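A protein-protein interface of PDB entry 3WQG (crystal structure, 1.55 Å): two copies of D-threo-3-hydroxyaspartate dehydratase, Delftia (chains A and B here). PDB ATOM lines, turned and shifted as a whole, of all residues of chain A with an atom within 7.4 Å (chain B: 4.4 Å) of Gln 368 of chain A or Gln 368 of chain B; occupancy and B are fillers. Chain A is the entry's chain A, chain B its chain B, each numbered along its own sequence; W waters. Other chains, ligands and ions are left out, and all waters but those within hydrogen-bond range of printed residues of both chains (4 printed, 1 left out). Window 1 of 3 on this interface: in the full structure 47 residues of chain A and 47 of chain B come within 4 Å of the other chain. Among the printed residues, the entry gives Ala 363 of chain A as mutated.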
ATOM      1  N   ALA A  23      18.776 -34.276  -3.615  1.00  0.00           N
ATOM      2  CA  ALA A  23      17.374 -34.358  -3.216  1.00  0.00           C
ATOM      3  C   ALA A  23      16.784 -35.537  -3.909  1.00  0.00           C
ATOM      4  O   ALA A  23      16.651 -35.542  -5.113  1.00  0.00           O
ATOM      5  CB  ALA A  23      16.663 -33.039  -3.556  1.00  0.00           C
ATOM      6  N   GLY A 289      24.225 -29.367   5.038  1.00  0.00           N
ATOM      7  CA  GLY A 289      23.937 -28.291   5.992  1.00  0.00           C
ATOM      8  C   GLY A 289      22.655 -27.577   5.654  1.00  0.00           C
ATOM      9  O   GLY A 289      21.783 -28.143   4.954  1.00  0.00           O
ATOM     10  N   TRP A 290      22.509 -26.359   6.148  1.00  0.00           N
ATOM     11  CA  TRP A 290      21.250 -25.623   5.895  1.00  0.00           C
ATOM     12  C   TRP A 290      21.175 -25.240   4.407  1.00  0.00           C
ATOM     13  O   TRP A 290      20.049 -24.980   3.911  1.00  0.00           O
ATOM     14  CB  TRP A 290      20.962 -24.451   6.817  1.00  0.00           C
ATOM     15  CG  TRP A 290      21.973 -23.338   6.727  1.00  0.00           C
ATOM     16  CD1 TRP A 290      22.934 -22.964   7.694  1.00  0.00           C
ATOM     17  CD2 TRP A 290      22.100 -22.323   5.630  1.00  0.00           C
ATOM     18  NE1 TRP A 290      23.596 -21.851   7.307  1.00  0.00           N
ATOM     19  CE2 TRP A 290      23.175 -21.422   6.037  1.00  0.00           C
ATOM     20  CE3 TRP A 290      21.418 -22.091   4.419  1.00  0.00           C
ATOM     21  CZ2 TRP A 290      23.534 -20.322   5.248  1.00  0.00           C
ATOM     22  CZ3 TRP A 290      21.844 -21.034   3.585  1.00  0.00           C
ATOM     23  CH2 TRP A 290      22.891 -20.174   4.001  1.00  0.00           C
ATOM     24  N   MET A 291      22.294 -25.133   3.657  1.00  0.00           N
ATOM     25  CA  MET A 291      22.102 -24.854   2.180  1.00  0.00           C
ATOM     26  C   MET A 291      21.379 -26.031   1.537  1.00  0.00           C
ATOM     27  O   MET A 291      20.612 -25.827   0.593  1.00  0.00           O
ATOM     28  CB  MET A 291      23.449 -24.640   1.510  1.00  0.00           C
ATOM     29  CG  MET A 291      23.332 -24.137   0.075  1.00  0.00           C
ATOM     30  SD  MET A 291      22.453 -22.511  -0.059  1.00  0.00           S
ATOM     31  CE  MET A 291      23.733 -21.395   0.556  1.00  0.00           C
ATOM     32  N   ALA A 292      21.584 -27.274   2.027  1.00  0.00           N
ATOM     33  CA  ALA A 292      20.825 -28.424   1.480  1.00  0.00           C
ATOM     34  C   ALA A 292      19.436 -28.482   2.152  1.00  0.00           C
ATOM     35  O   ALA A 292      18.437 -28.706   1.440  1.00  0.00           O
ATOM     36  CB  ALA A 292      21.588 -29.715   1.776  1.00  0.00           C
ATOM     37  N   MET A 293      19.350 -28.386   3.479  1.00  0.00           N
ATOM     38  CA  MET A 293      18.040 -28.627   4.112  1.00  0.00           C
ATOM     39  C   MET A 293      17.070 -27.409   4.047  1.00  0.00           C
ATOM     40  O   MET A 293      15.856 -27.586   4.258  1.00  0.00           O
ATOM     41  CB  MET A 293      18.202 -29.016   5.597  1.00  0.00           C
ATOM     42  CG  MET A 293      19.060 -30.263   5.842  1.00  0.00           C
ATOM     43  SD  MET A 293      18.663 -31.684   4.769  1.00  0.00           S
ATOM     44  CE  MET A 293      16.909 -31.967   5.226  1.00  0.00           C
ATOM     45  N   SER A 294      17.672 -26.213   3.821  1.00  0.00           N
ATOM     46  CA  SER A 294      17.075 -24.908   4.062  1.00  0.00           C
ATOM     47  C   SER A 294      17.137 -24.605   5.559  1.00  0.00           C
ATOM     48  O   SER A 294      17.316 -25.509   6.401  1.00  0.00           O
ATOM     49  CB  SER A 294      15.589 -24.801   3.546  1.00  0.00           C
ATOM     50  OG  SER A 294      14.656 -25.223   4.515  1.00  0.00           O
ATOM     51  N   ARG A 295      16.875 -23.352   5.871  1.00  0.00           N
ATOM     52  CA  ARG A 295      16.809 -22.895   7.285  1.00  0.00           C
ATOM     53  C   ARG A 295      15.436 -23.223   7.923  1.00  0.00           C
ATOM     54  O   ARG A 295      15.207 -22.823   9.041  1.00  0.00           O
ATOM     55  CB  ARG A 295      17.018 -21.408   7.304  1.00  0.00           C
ATOM     56  CG  ARG A 295      18.528 -21.103   7.218  1.00  0.00           C
ATOM     57  CD  ARG A 295      19.105 -21.537   8.612  1.00  0.00           C
ATOM     58  NE  ARG A 295      20.149 -20.639   9.049  1.00  0.00           N
ATOM     59  CZ  ARG A 295      21.136 -20.937   9.885  1.00  0.00           C
ATOM     60  NH1 ARG A 295      21.175 -22.096  10.481  1.00  0.00           N
ATOM     61  NH2 ARG A 295      22.064 -20.005  10.149  1.00  0.00           N
ATOM     62  N   ALA A 362       8.973 -29.742   2.970  1.00  0.00           N
ATOM     63  CA  ALA A 362       9.405 -30.265   1.669  1.00  0.00           C
ATOM     64  C   ALA A 362       9.599 -29.115   0.673  1.00  0.00           C
ATOM     65  O   ALA A 362      10.554 -29.190  -0.141  1.00  0.00           O
ATOM     66  CB  ALA A 362       8.386 -31.291   1.128  1.00  0.00           C
ATOM     67  N   ALA A 363       8.719 -28.093   0.643  1.00  0.00           N
ATOM     68  CA  ALA A 363       8.872 -27.046  -0.430  1.00  0.00           C
ATOM     69  C   ALA A 363      10.165 -26.233  -0.175  1.00  0.00           C
ATOM     70  O   ALA A 363      10.844 -25.771  -1.150  1.00  0.00           O
ATOM     71  CB  ALA A 363       7.661 -26.106  -0.371  1.00  0.00           C
ATOM     72  N   ALA A 364      10.518 -26.023   1.109  1.00  0.00           N
ATOM     73  CA  ALA A 364      11.706 -25.204   1.404  1.00  0.00           C
ATOM     74  C   ALA A 364      12.969 -26.011   1.046  1.00  0.00           C
ATOM     75  O   ALA A 364      13.900 -25.468   0.435  1.00  0.00           O
ATOM     76  CB  ALA A 364      11.747 -24.825   2.881  1.00  0.00           C
ATOM     77  N   THR A 365      13.031 -27.294   1.455  1.00  0.00           N
ATOM     78  CA  THR A 365      14.210 -28.080   1.153  1.00  0.00           C
ATOM     79  C   THR A 365      14.335 -28.256  -0.382  1.00  0.00           C
ATOM     80  O   THR A 365      15.417 -28.090  -0.955  1.00  0.00           O
ATOM     81  CB  THR A 365      14.058 -29.483   1.815  1.00  0.00           C
ATOM     82  OG1 THR A 365      14.145 -29.264   3.226  1.00  0.00           O
ATOM     83  CG2 THR A 365      15.244 -30.415   1.365  1.00  0.00           C
ATOM     84  N   GLY A 366      13.210 -28.578  -1.058  1.00  0.00           N
ATOM     85  CA  GLY A 366      13.302 -28.830  -2.545  1.00  0.00           C
ATOM     86  C   GLY A 366      13.846 -27.585  -3.235  1.00  0.00           C
ATOM     87  O   GLY A 366      14.578 -27.770  -4.246  1.00  0.00           O
ATOM     88  N   ALA A 367      13.444 -26.345  -2.794  1.00  0.00           N
ATOM     89  CA  ALA A 367      13.907 -25.179  -3.516  1.00  0.00           C
ATOM     90  C   ALA A 367      15.409 -24.923  -3.405  1.00  0.00           C
ATOM     91  O   ALA A 367      15.974 -24.123  -4.202  1.00  0.00           O
ATOM     92  CB  ALA A 367      13.188 -23.926  -2.984  1.00  0.00           C
ATOM     93  N   GLN A 368      16.097 -25.673  -2.531  1.00  0.00           N
ATOM     94  CA  GLN A 368      17.561 -25.546  -2.465  1.00  0.00           C
ATOM     95  C   GLN A 368      18.280 -26.283  -3.582  1.00  0.00           C
ATOM     96  O   GLN A 368      19.504 -26.093  -3.751  1.00  0.00           O
ATOM     97  CB  GLN A 368      18.039 -26.042  -1.100  1.00  0.00           C
ATOM     98  CG  GLN A 368      17.407 -25.233   0.068  1.00  0.00           C
ATOM     99  CD  GLN A 368      17.729 -23.771  -0.009  1.00  0.00           C
ATOM    100  OE1 GLN A 368      17.026 -22.996  -0.650  1.00  0.00           O
ATOM    101  NE2 GLN A 368      18.801 -23.360   0.658  1.00  0.00           N
ATOM    102  N   PHE A 369      17.557 -27.096  -4.384  1.00  0.00           N
ATOM    103  CA  PHE A 369      18.208 -27.972  -5.358  1.00  0.00           C
ATOM    104  C   PHE A 369      17.793 -27.590  -6.775  1.00  0.00           C
ATOM    105  O   PHE A 369      16.574 -27.416  -7.059  1.00  0.00           O
ATOM    106  CB  PHE A 369      17.808 -29.460  -5.130  1.00  0.00           C
ATOM    107  CG  PHE A 369      18.423 -29.998  -3.843  1.00  0.00           C
ATOM    108  CD1 PHE A 369      17.768 -29.783  -2.600  1.00  0.00           C
ATOM    109  CD2 PHE A 369      19.698 -30.633  -3.903  1.00  0.00           C
ATOM    110  CE1 PHE A 369      18.380 -30.193  -1.428  1.00  0.00           C
ATOM    111  CE2 PHE A 369      20.269 -31.113  -2.689  1.00  0.00           C
ATOM    112  CZ  PHE A 369      19.624 -30.843  -1.483  1.00  0.00           C
ATOM    113  N   PRO A 370      18.734 -27.619  -7.722  1.00  0.00           N
ATOM    114  CA  PRO A 370      18.367 -27.437  -9.153  1.00  0.00           C
ATOM    115  C   PRO A 370      17.499 -28.561  -9.698  1.00  0.00           C
ATOM    116  O   PRO A 370      16.826 -28.360 -10.720  1.00  0.00           O
ATOM    117  CB  PRO A 370      19.733 -27.464  -9.855  1.00  0.00           C
ATOM    118  CG  PRO A 370      20.745 -27.051  -8.769  1.00  0.00           C
ATOM    119  CD  PRO A 370      20.216 -27.564  -7.478  1.00  0.00           C
ATOM    120  N   ALA A 371      17.528 -29.753  -9.057  1.00  0.00           N
ATOM    121  CA  ALA A 371      16.859 -30.927  -9.563  1.00  0.00           C
ATOM    122  C   ALA A 371      16.670 -31.942  -8.456  1.00  0.00           C
ATOM    123  O   ALA A 371      17.394 -31.930  -7.409  1.00  0.00           O
ATOM    124  CB  ALA A 371      17.633 -31.601 -10.720  1.00  0.00           C
ATOM    125  N   TYR A 372      15.679 -32.810  -8.678  1.00  0.00           N
ATOM    126  CA  TYR A 372      15.514 -34.001  -7.868  1.00  0.00           C
ATOM    127  C   TYR A 372      16.135 -35.187  -8.537  1.00  0.00           C
ATOM    128  O   TYR A 372      16.311 -35.238  -9.757  1.00  0.00           O
ATOM    129  CB  TYR A 372      14.009 -34.351  -7.691  1.00  0.00           C
ATOM    130  CG  TYR A 372      13.226 -33.231  -7.022  1.00  0.00           C
ATOM    131  CD1 TYR A 372      13.220 -33.084  -5.597  1.00  0.00           C
ATOM    132  CD2 TYR A 372      12.431 -32.317  -7.791  1.00  0.00           C
ATOM    133  CE1 TYR A 372      12.461 -32.092  -4.957  1.00  0.00           C
ATOM    134  CE2 TYR A 372      11.690 -31.304  -7.153  1.00  0.00           C
ATOM    135  CZ  TYR A 372      11.699 -31.170  -5.730  1.00  0.00           C
ATOM    136  OH  TYR A 372      11.032 -30.159  -5.104  1.00  0.00           O
ATOM    137  N   ARG A 386      13.942 -28.855 -11.579  1.00  0.00           N
ATOM    138  CA  ARG A 386      12.891 -28.044 -11.055  1.00  0.00           C
ATOM    139  C   ARG A 386      13.289 -26.574 -11.157  1.00  0.00           C
ATOM    140  O   ARG A 386      14.474 -26.238 -11.416  1.00  0.00           O
ATOM    141  CB  ARG A 386      12.534 -28.460  -9.601  1.00  0.00           C
ATOM    142  CG  ARG A 386      13.739 -28.244  -8.661  1.00  0.00           C
ATOM    143  CD  ARG A 386      13.259 -28.051  -7.227  1.00  0.00           C
ATOM    144  NE  ARG A 386      12.658 -26.684  -7.106  1.00  0.00           N
ATOM    145  CZ  ARG A 386      11.745 -26.349  -6.187  1.00  0.00           C
ATOM    146  NH1 ARG A 386      11.408 -25.066  -6.088  1.00  0.00           N
ATOM    147  NH2 ARG A 386      11.132 -27.261  -5.397  1.00  0.00           N
ATOM    148  N   LEU A 387      12.334 -25.674 -10.929  1.00  0.00           N
ATOM    149  CA  LEU A 387      12.518 -24.232 -11.200  1.00  0.00           C
ATOM    150  C   LEU A 387      13.081 -23.549  -9.934  1.00  0.00           C
ATOM    151  O   LEU A 387      12.721 -23.904  -8.808  1.00  0.00           O
ATOM    152  CB  LEU A 387      11.115 -23.634 -11.520  1.00  0.00           C
ATOM    153  CG  LEU A 387      11.106 -22.297 -12.259  1.00  0.00           C
ATOM    154  CD1 LEU A 387      11.597 -22.584 -13.764  1.00  0.00           C
ATOM    155  CD2 LEU A 387       9.623 -21.921 -12.278  1.00  0.00           C
ATOM    156  N   HIS A 388      13.909 -22.526 -10.186  1.00  0.00           N
ATOM    157  CA  HIS A 388      14.444 -21.626  -9.193  1.00  0.00           C
ATOM    158  C   HIS A 388      14.156 -20.207  -9.637  1.00  0.00           C
ATOM    159  O   HIS A 388      14.404 -19.897 -10.832  1.00  0.00           O
ATOM    160  CB  HIS A 388      15.988 -21.896  -9.137  1.00  0.00           C
ATOM    161  CG  HIS A 388      16.718 -21.148  -8.044  1.00  0.00           C
ATOM    162  ND1 HIS A 388      17.946 -20.542  -8.274  1.00  0.00           N
ATOM    163  CD2 HIS A 388      16.435 -21.028  -6.716  1.00  0.00           C
ATOM    164  CE1 HIS A 388      18.390 -20.052  -7.028  1.00  0.00           C
ATOM    165  NE2 HIS A 388      17.456 -20.374  -6.103  1.00  0.00           N
ATOM    166  N   GLY A 389      13.803 -19.330  -8.706  1.00  0.00           N
ATOM    167  CA  GLY A 389      13.657 -17.925  -9.023  1.00  0.00           C
ATOM    168  C   GLY A 389      12.309 -17.493  -9.564  1.00  0.00           C
ATOM    169  O   GLY A 389      11.298 -18.102  -9.308  1.00  0.00           O
ATOM    170  N   TRP A 390      12.311 -16.316 -10.186  1.00  0.00           N
ATOM    171  CA  TRP A 390      11.092 -15.579 -10.580  1.00  0.00           C
ATOM    172  C   TRP A 390      11.215 -15.151 -11.999  1.00  0.00           C
ATOM    173  O   TRP A 390      12.304 -15.137 -12.629  1.00  0.00           O
ATOM    174  CB  TRP A 390      10.920 -14.313  -9.676  1.00  0.00           C
ATOM    175  CG  TRP A 390      10.612 -14.697  -8.268  1.00  0.00           C
ATOM    176  CD1 TRP A 390       9.367 -14.883  -7.698  1.00  0.00           C
ATOM    177  CD2 TRP A 390      11.593 -15.066  -7.223  1.00  0.00           C
ATOM    178  NE1 TRP A 390       9.459 -15.327  -6.378  1.00  0.00           N
ATOM    179  CE2 TRP A 390      10.808 -15.446  -6.036  1.00  0.00           C
ATOM    180  CE3 TRP A 390      13.025 -15.050  -7.134  1.00  0.00           C
ATOM    181  CZ2 TRP A 390      11.435 -15.870  -4.838  1.00  0.00           C
ATOM    182  CZ3 TRP A 390      13.607 -15.490  -5.907  1.00  0.00           C
ATOM    183  CH2 TRP A 390      12.866 -15.897  -4.828  1.00  0.00           C
ATOM    184  OXT TRP A 390      10.181 -14.718 -12.551  1.00  0.00           O
ATOM    185  N   TRP B 290       9.101 -16.149   2.351  1.00  0.00           N
ATOM    186  CA  TRP B 290      10.372 -16.817   2.716  1.00  0.00           C
ATOM    187  C   TRP B 290      11.087 -17.414   1.529  1.00  0.00           C
ATOM    188  O   TRP B 290      12.304 -17.616   1.563  1.00  0.00           O
ATOM    189  CB  TRP B 290      10.171 -17.839   3.832  1.00  0.00           C
ATOM    190  CG  TRP B 290       9.256 -19.014   3.480  1.00  0.00           C
ATOM    191  CD1 TRP B 290       7.963 -19.285   3.967  1.00  0.00           C
ATOM    192  CD2 TRP B 290       9.566 -20.165   2.567  1.00  0.00           C
ATOM    193  NE1 TRP B 290       7.490 -20.441   3.448  1.00  0.00           N
ATOM    194  CE2 TRP B 290       8.399 -21.005   2.576  1.00  0.00           C
ATOM    195  CE3 TRP B 290      10.714 -20.586   1.802  1.00  0.00           C
ATOM    196  CZ2 TRP B 290       8.370 -22.219   1.845  1.00  0.00           C
ATOM    197  CZ3 TRP B 290      10.628 -21.745   1.003  1.00  0.00           C
ATOM    198  CH2 TRP B 290       9.479 -22.543   1.047  1.00  0.00           C
ATOM    199  N   MET B 291      10.369 -17.671   0.396  1.00  0.00           N
ATOM    200  CA  MET B 291      11.124 -18.041  -0.808  1.00  0.00           C
ATOM    201  C   MET B 291      12.111 -16.964  -1.237  1.00  0.00           C
ATOM    202  O   MET B 291      13.187 -17.294  -1.735  1.00  0.00           O
ATOM    203  CB  MET B 291      10.191 -18.502  -1.943  1.00  0.00           C
ATOM    204  CG  MET B 291      10.939 -19.175  -3.164  1.00  0.00           C
ATOM    205  SD  MET B 291      11.756 -20.748  -2.658  1.00  0.00           S
ATOM    206  CE  MET B 291      10.295 -21.807  -2.513  1.00  0.00           C
ATOM    207  N   ALA B 292      11.773 -15.661  -1.069  1.00  0.00           N
ATOM    208  CA  ALA B 292      12.697 -14.606  -1.369  1.00  0.00           C
ATOM    209  C   ALA B 292      13.669 -14.379  -0.202  1.00  0.00           C
ATOM    210  O   ALA B 292      14.880 -14.212  -0.459  1.00  0.00           O
ATOM    211  CB  ALA B 292      11.912 -13.317  -1.639  1.00  0.00           C
ATOM    212  N   SER B 294      14.497 -16.309   2.397  1.00  0.00           N
ATOM    213  CA  SER B 294      14.859 -17.550   3.048  1.00  0.00           C
ATOM    214  C   SER B 294      14.178 -17.629   4.404  1.00  0.00           C
ATOM    215  O   SER B 294      13.600 -16.636   4.962  1.00  0.00           O
ATOM    216  CB  SER B 294      16.427 -17.738   3.250  1.00  0.00           C
ATOM    217  OG  SER B 294      16.826 -17.110   4.482  1.00  0.00           O
ATOM    218  N   ALA B 364      22.084 -16.718   3.129  1.00  0.00           N
ATOM    219  CA  ALA B 364      20.804 -17.501   3.000  1.00  0.00           C
ATOM    220  C   ALA B 364      19.843 -16.830   2.029  1.00  0.00           C
ATOM    221  O   ALA B 364      19.291 -17.448   1.097  1.00  0.00           O
ATOM    222  CB  ALA B 364      20.129 -17.754   4.368  1.00  0.00           C
ATOM    223  N   THR B 365      19.679 -15.522   2.185  1.00  0.00           N
ATOM    224  CA  THR B 365      18.803 -14.759   1.205  1.00  0.00           C
ATOM    225  C   THR B 365      19.391 -14.802  -0.204  1.00  0.00           C
ATOM    226  O   THR B 365      18.619 -15.088  -1.164  1.00  0.00           O
ATOM    227  CB  THR B 365      18.660 -13.287   1.662  1.00  0.00           C
ATOM    228  OG1 THR B 365      18.002 -13.274   2.915  1.00  0.00           O
ATOM    229  CG2 THR B 365      17.898 -12.440   0.581  1.00  0.00           C
ATOM    230  N   GLY B 366      20.726 -14.578  -0.375  1.00  0.00           N
ATOM    231  CA  GLY B 366      21.266 -14.580  -1.724  1.00  0.00           C
ATOM    232  C   GLY B 366      21.027 -15.910  -2.454  1.00  0.00           C
ATOM    233  O   GLY B 366      20.810 -15.893  -3.686  1.00  0.00           O
ATOM    234  N   ALA B 367      21.121 -17.023  -1.713  1.00  0.00           N
ATOM    235  CA  ALA B 367      21.004 -18.326  -2.367  1.00  0.00           C
ATOM    236  C   ALA B 367      19.578 -18.566  -2.951  1.00  0.00           C
ATOM    237  O   ALA B 367      19.390 -19.499  -3.739  1.00  0.00           O
ATOM    238  CB  ALA B 367      21.347 -19.437  -1.351  1.00  0.00           C
ATOM    239  N   GLN B 368      18.608 -17.767  -2.550  1.00  0.00           N
ATOM    240  CA  GLN B 368      17.242 -17.897  -3.093  1.00  0.00           C
ATOM    241  C   GLN B 368      17.131 -17.367  -4.509  1.00  0.00           C
ATOM    242  O   GLN B 368      16.120 -17.602  -5.191  1.00  0.00           O
ATOM    243  CB  GLN B 368      16.276 -17.189  -2.164  1.00  0.00           C
ATOM    244  CG  GLN B 368      16.283 -17.846  -0.806  1.00  0.00           C
ATOM    245  CD  GLN B 368      16.015 -19.354  -0.852  1.00  0.00           C
ATOM    246  OE1 GLN B 368      16.943 -20.168  -0.823  1.00  0.00           O
ATOM    247  NE2 GLN B 368      14.767 -19.732  -1.059  1.00  0.00           N
ATOM    248  N   PHE B 369      18.165 -16.662  -4.983  1.00  0.00           N
ATOM    249  CA  PHE B 369      18.057 -15.997  -6.292  1.00  0.00           C
ATOM    250  C   PHE B 369      19.041 -16.548  -7.336  1.00  0.00           C
ATOM    251  O   PHE B 369      20.221 -16.718  -7.033  1.00  0.00           O
ATOM    252  CB  PHE B 369      18.325 -14.468  -6.169  1.00  0.00           C
ATOM    253  CG  PHE B 369      17.274 -13.788  -5.360  1.00  0.00           C
ATOM    254  CD1 PHE B 369      17.296 -13.793  -3.945  1.00  0.00           C
ATOM    255  CD2 PHE B 369      16.184 -13.171  -6.002  1.00  0.00           C
ATOM    256  CE1 PHE B 369      16.277 -13.192  -3.187  1.00  0.00           C
ATOM    257  CE2 PHE B 369      15.163 -12.602  -5.267  1.00  0.00           C
ATOM    258  CZ  PHE B 369      15.213 -12.558  -3.856  1.00  0.00           C
ATOM    259  N   PRO B 370      18.616 -16.721  -8.591  1.00  0.00           N
ATOM    260  CA  PRO B 370      19.534 -17.074  -9.698  1.00  0.00           C
ATOM    261  C   PRO B 370      20.561 -16.012  -9.923  1.00  0.00           C
ATOM    262  O   PRO B 370      21.629 -16.338 -10.404  1.00  0.00           O
ATOM    263  CB  PRO B 370      18.607 -17.188 -10.929  1.00  0.00           C
ATOM    264  CG  PRO B 370      17.233 -17.539 -10.355  1.00  0.00           C
ATOM    265  CD  PRO B 370      17.171 -16.789  -9.006  1.00  0.00           C
ATOM    266  N   HIS B 388      23.800 -21.825  -8.037  1.00  0.00           N
ATOM    267  CA  HIS B 388      22.818 -22.601  -7.243  1.00  0.00           C
ATOM    268  C   HIS B 388      23.157 -24.066  -7.304  1.00  0.00           C
ATOM    269  O   HIS B 388      23.449 -24.573  -8.357  1.00  0.00           O
ATOM    270  CB  HIS B 388      21.421 -22.352  -7.904  1.00  0.00           C
ATOM    271  CG  HIS B 388      20.291 -22.968  -7.140  1.00  0.00           C
ATOM    272  ND1 HIS B 388      19.263 -23.725  -7.736  1.00  0.00           N
ATOM    273  CD2 HIS B 388      19.983 -22.854  -5.815  1.00  0.00           C
ATOM    274  CE1 HIS B 388      18.358 -24.011  -6.761  1.00  0.00           C
ATOM    275  NE2 HIS B 388      18.786 -23.449  -5.599  1.00  0.00           N
ATOM    276  N   TRP B 390      25.039 -27.918  -6.357  1.00  0.00           N
ATOM    277  CA  TRP B 390      26.330 -28.575  -6.129  1.00  0.00           C
ATOM    278  C   TRP B 390      26.879 -29.164  -7.411  1.00  0.00           C
ATOM    279  O   TRP B 390      26.224 -29.055  -8.505  1.00  0.00           O
ATOM    280  CB  TRP B 390      26.155 -29.703  -5.075  1.00  0.00           C
ATOM    281  CG  TRP B 390      25.776 -29.140  -3.721  1.00  0.00           C
ATOM    282  CD1 TRP B 390      26.637 -28.838  -2.692  1.00  0.00           C
ATOM    283  CD2 TRP B 390      24.422 -28.724  -3.233  1.00  0.00           C
ATOM    284  NE1 TRP B 390      25.959 -28.302  -1.623  1.00  0.00           N
ATOM    285  CE2 TRP B 390      24.603 -28.191  -1.902  1.00  0.00           C
ATOM    286  CE3 TRP B 390      23.111 -28.739  -3.799  1.00  0.00           C
ATOM    287  CZ2 TRP B 390      23.544 -27.652  -1.143  1.00  0.00           C
ATOM    288  CZ3 TRP B 390      22.062 -28.193  -2.998  1.00  0.00           C
ATOM    289  CH2 TRP B 390      22.289 -27.638  -1.725  1.00  0.00           C
ATOM    290  OXT TRP B 390      27.973 -29.830  -7.347  1.00  0.00           O
HETATM  291  O   HOH W   1      11.717 -22.042  -6.003  1.00  0.00           O
HETATM  292  O   HOH W   2      14.404 -22.738   0.274  1.00  0.00           O
HETATM  293  O   HOH W   3      16.013 -21.319  -3.562  1.00  0.00           O
HETATM  294  O   HOH W   4      18.829 -20.225   1.143  1.00  0.00           O
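O of Ala 367 of chain A is in hydrogen-bond range of NE2 of His 388 of chain B, 3.2 Å away.
The side-chain amide oxygen (OE1) of Gln 368 of chain A lies close to the side-chain amide oxygen (OE1) of Gln 368 of chain B (2.8 Å).
A ring nitrogen (NE2) of His 388 of chain B is in hydrogen-bond range of the backbone carbonyl oxygen (O) of Gln 368 of chain A.
A ring nitrogen (NE2) of His 388 of chain A sits at hydrogen-bond distance from the backbone carbonyl oxygen (O) of Ala 367 of chain B (3.2 Å).
A ring nitrogen (NE2) of His 388 of chain A is in hydrogen-bond range of the backbone carbonyl oxygen (O) of Gln 368 of chain B (3.2 Å).
NE2 of His 388 of chain B is in hydrogen-bond range of NE2 of His 388 of chain A (3.4 Å).
The backbone carbonyl oxygen (O) of Met 291 of chain A is in hydrogen-bond range of the side-chain amide nitrogen (NE2) of Gln 368 of chain A.
The backbone carbonyl oxygen (O) of Pro 370 of chain A is in hydrogen-bond range of the backbone NH (N) of Arg 386 of chain A, at 3.0 Å.
The side-chain amide nitrogen (NE2) of Gln 368 of chain B is in hydrogen-bond range of the backbone carbonyl oxygen (O) of Met 291 of chain B (3.0 Å).
Trp 290 of chain A touches Ala 364 of chain B (CH2 to CA, 3.5 Å).
CB of Ala 367 of chain B touches SD of Met 291 of chain A, 3.5 Å away.
CH2 of Trp 290 of chain B touches C of Ala 363 of chain A, at 3.9 Å.
Ala 364 of chain A touches Trp 290 of chain B.
Trp 390 of chain B touches Phe 369 of chain A.
Pro 370 of chain A touches His 388 of chain B (CG to O, 3.7 Å).
His 388 of chain A touches Phe 369 of chain B (CE1 to C, 3.6 Å).
N of Pro 370 of chain B touches CE1 of His 388 of chain A, at 3.7 Å.
Met 291 of chain B touches Trp 390 of chain A (O to CH2, 3.4 Å).
Gln 368 of chain B touches Trp 390 of chain A (O to CZ3, 3.4 Å).
Of the printed residues of chain B, Gln 368 of chain A touches Gln 368 (2.8 Å), His 388 (3.3 Å) and Trp 390 (3.4 Å).
Printed residues of chain A within 4 Å of Gln 368 of chain B: Gln 368, His 388 and Trp 390.
Printed residues of chain B within 4 Å of Trp 390 of chain A: Met 291, Ala 292, Gln 368 and Phe 369.
Of the printed residues of chain A, Ala 364 of chain B touches Trp 290 (3.5 Å).
Printed residues of chain B within 4 Å of Met 291 of chain A: Ala 367 and Trp 390.
Printed residues of chain A within 4 Å of Met 291 of chain B: Ala 367 and Trp 390.
Ser 294 of chain B touches none of the printed residues of chain A.
The nearest printed residue of chain B that does not touch Gln 368 of chain A is Ala 367 of chain B (5.1 Å).
The nearest printed residue of chain A that does not touch Gln 368 of chain B is Gly 389 of chain A (4.6 Å).
Of the 13 printed residues of chain B, 10 touch a printed residue of chain A.
Along chain B the printed residues that touch a printed residue of chain A span positions 290 to 390.
Of the 24 printed residues of chain A, 12 touch a printed residue of chain B.
Among the printed residues, no Asp or Glu carboxylate lies within 4 Å of a Lys or Arg side-chain nitrogen of the other chain.
Gln 368 of chain A touches His 388 of chain B, and with the chains exchanged His 388 of chain A touches Gln 368 of chain B.
Gln 368 of chain A touches Trp 390 of chain B, and with the chains exchanged Trp 390 of chain A touches Gln 368 of chain B.
Pro 370 of chain A touches His 388 of chain B, and with the chains exchanged His 388 of chain A touches Pro 370 of chain B.
Of the 24 pairs that touch across the chains among the printed residues, 22 have their exchanged pair printed and touching as well.
Water W4 lies within hydrogen-bond range of OE1 of Gln 368 of chain B (2.7 Å), O of Ala 364 of chain B (2.8 Å) and NE2 of Gln 368 of chain A (3.2 Å).
Water W3 lies within hydrogen-bond range of the backbone carbonyl oxygen (O) of Ala 367 of chain A, a ring nitrogen (NE2) of His 388 of chain A and the side-chain amide oxygen (OE1) of Gln 368 of chain B.
Water W1 lies within hydrogen-bond range of the guanidinium group of Arg 386 of chain A (3.0 Å) and the side-chain sulfur of Met 291 of chain B (3.6 Å).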
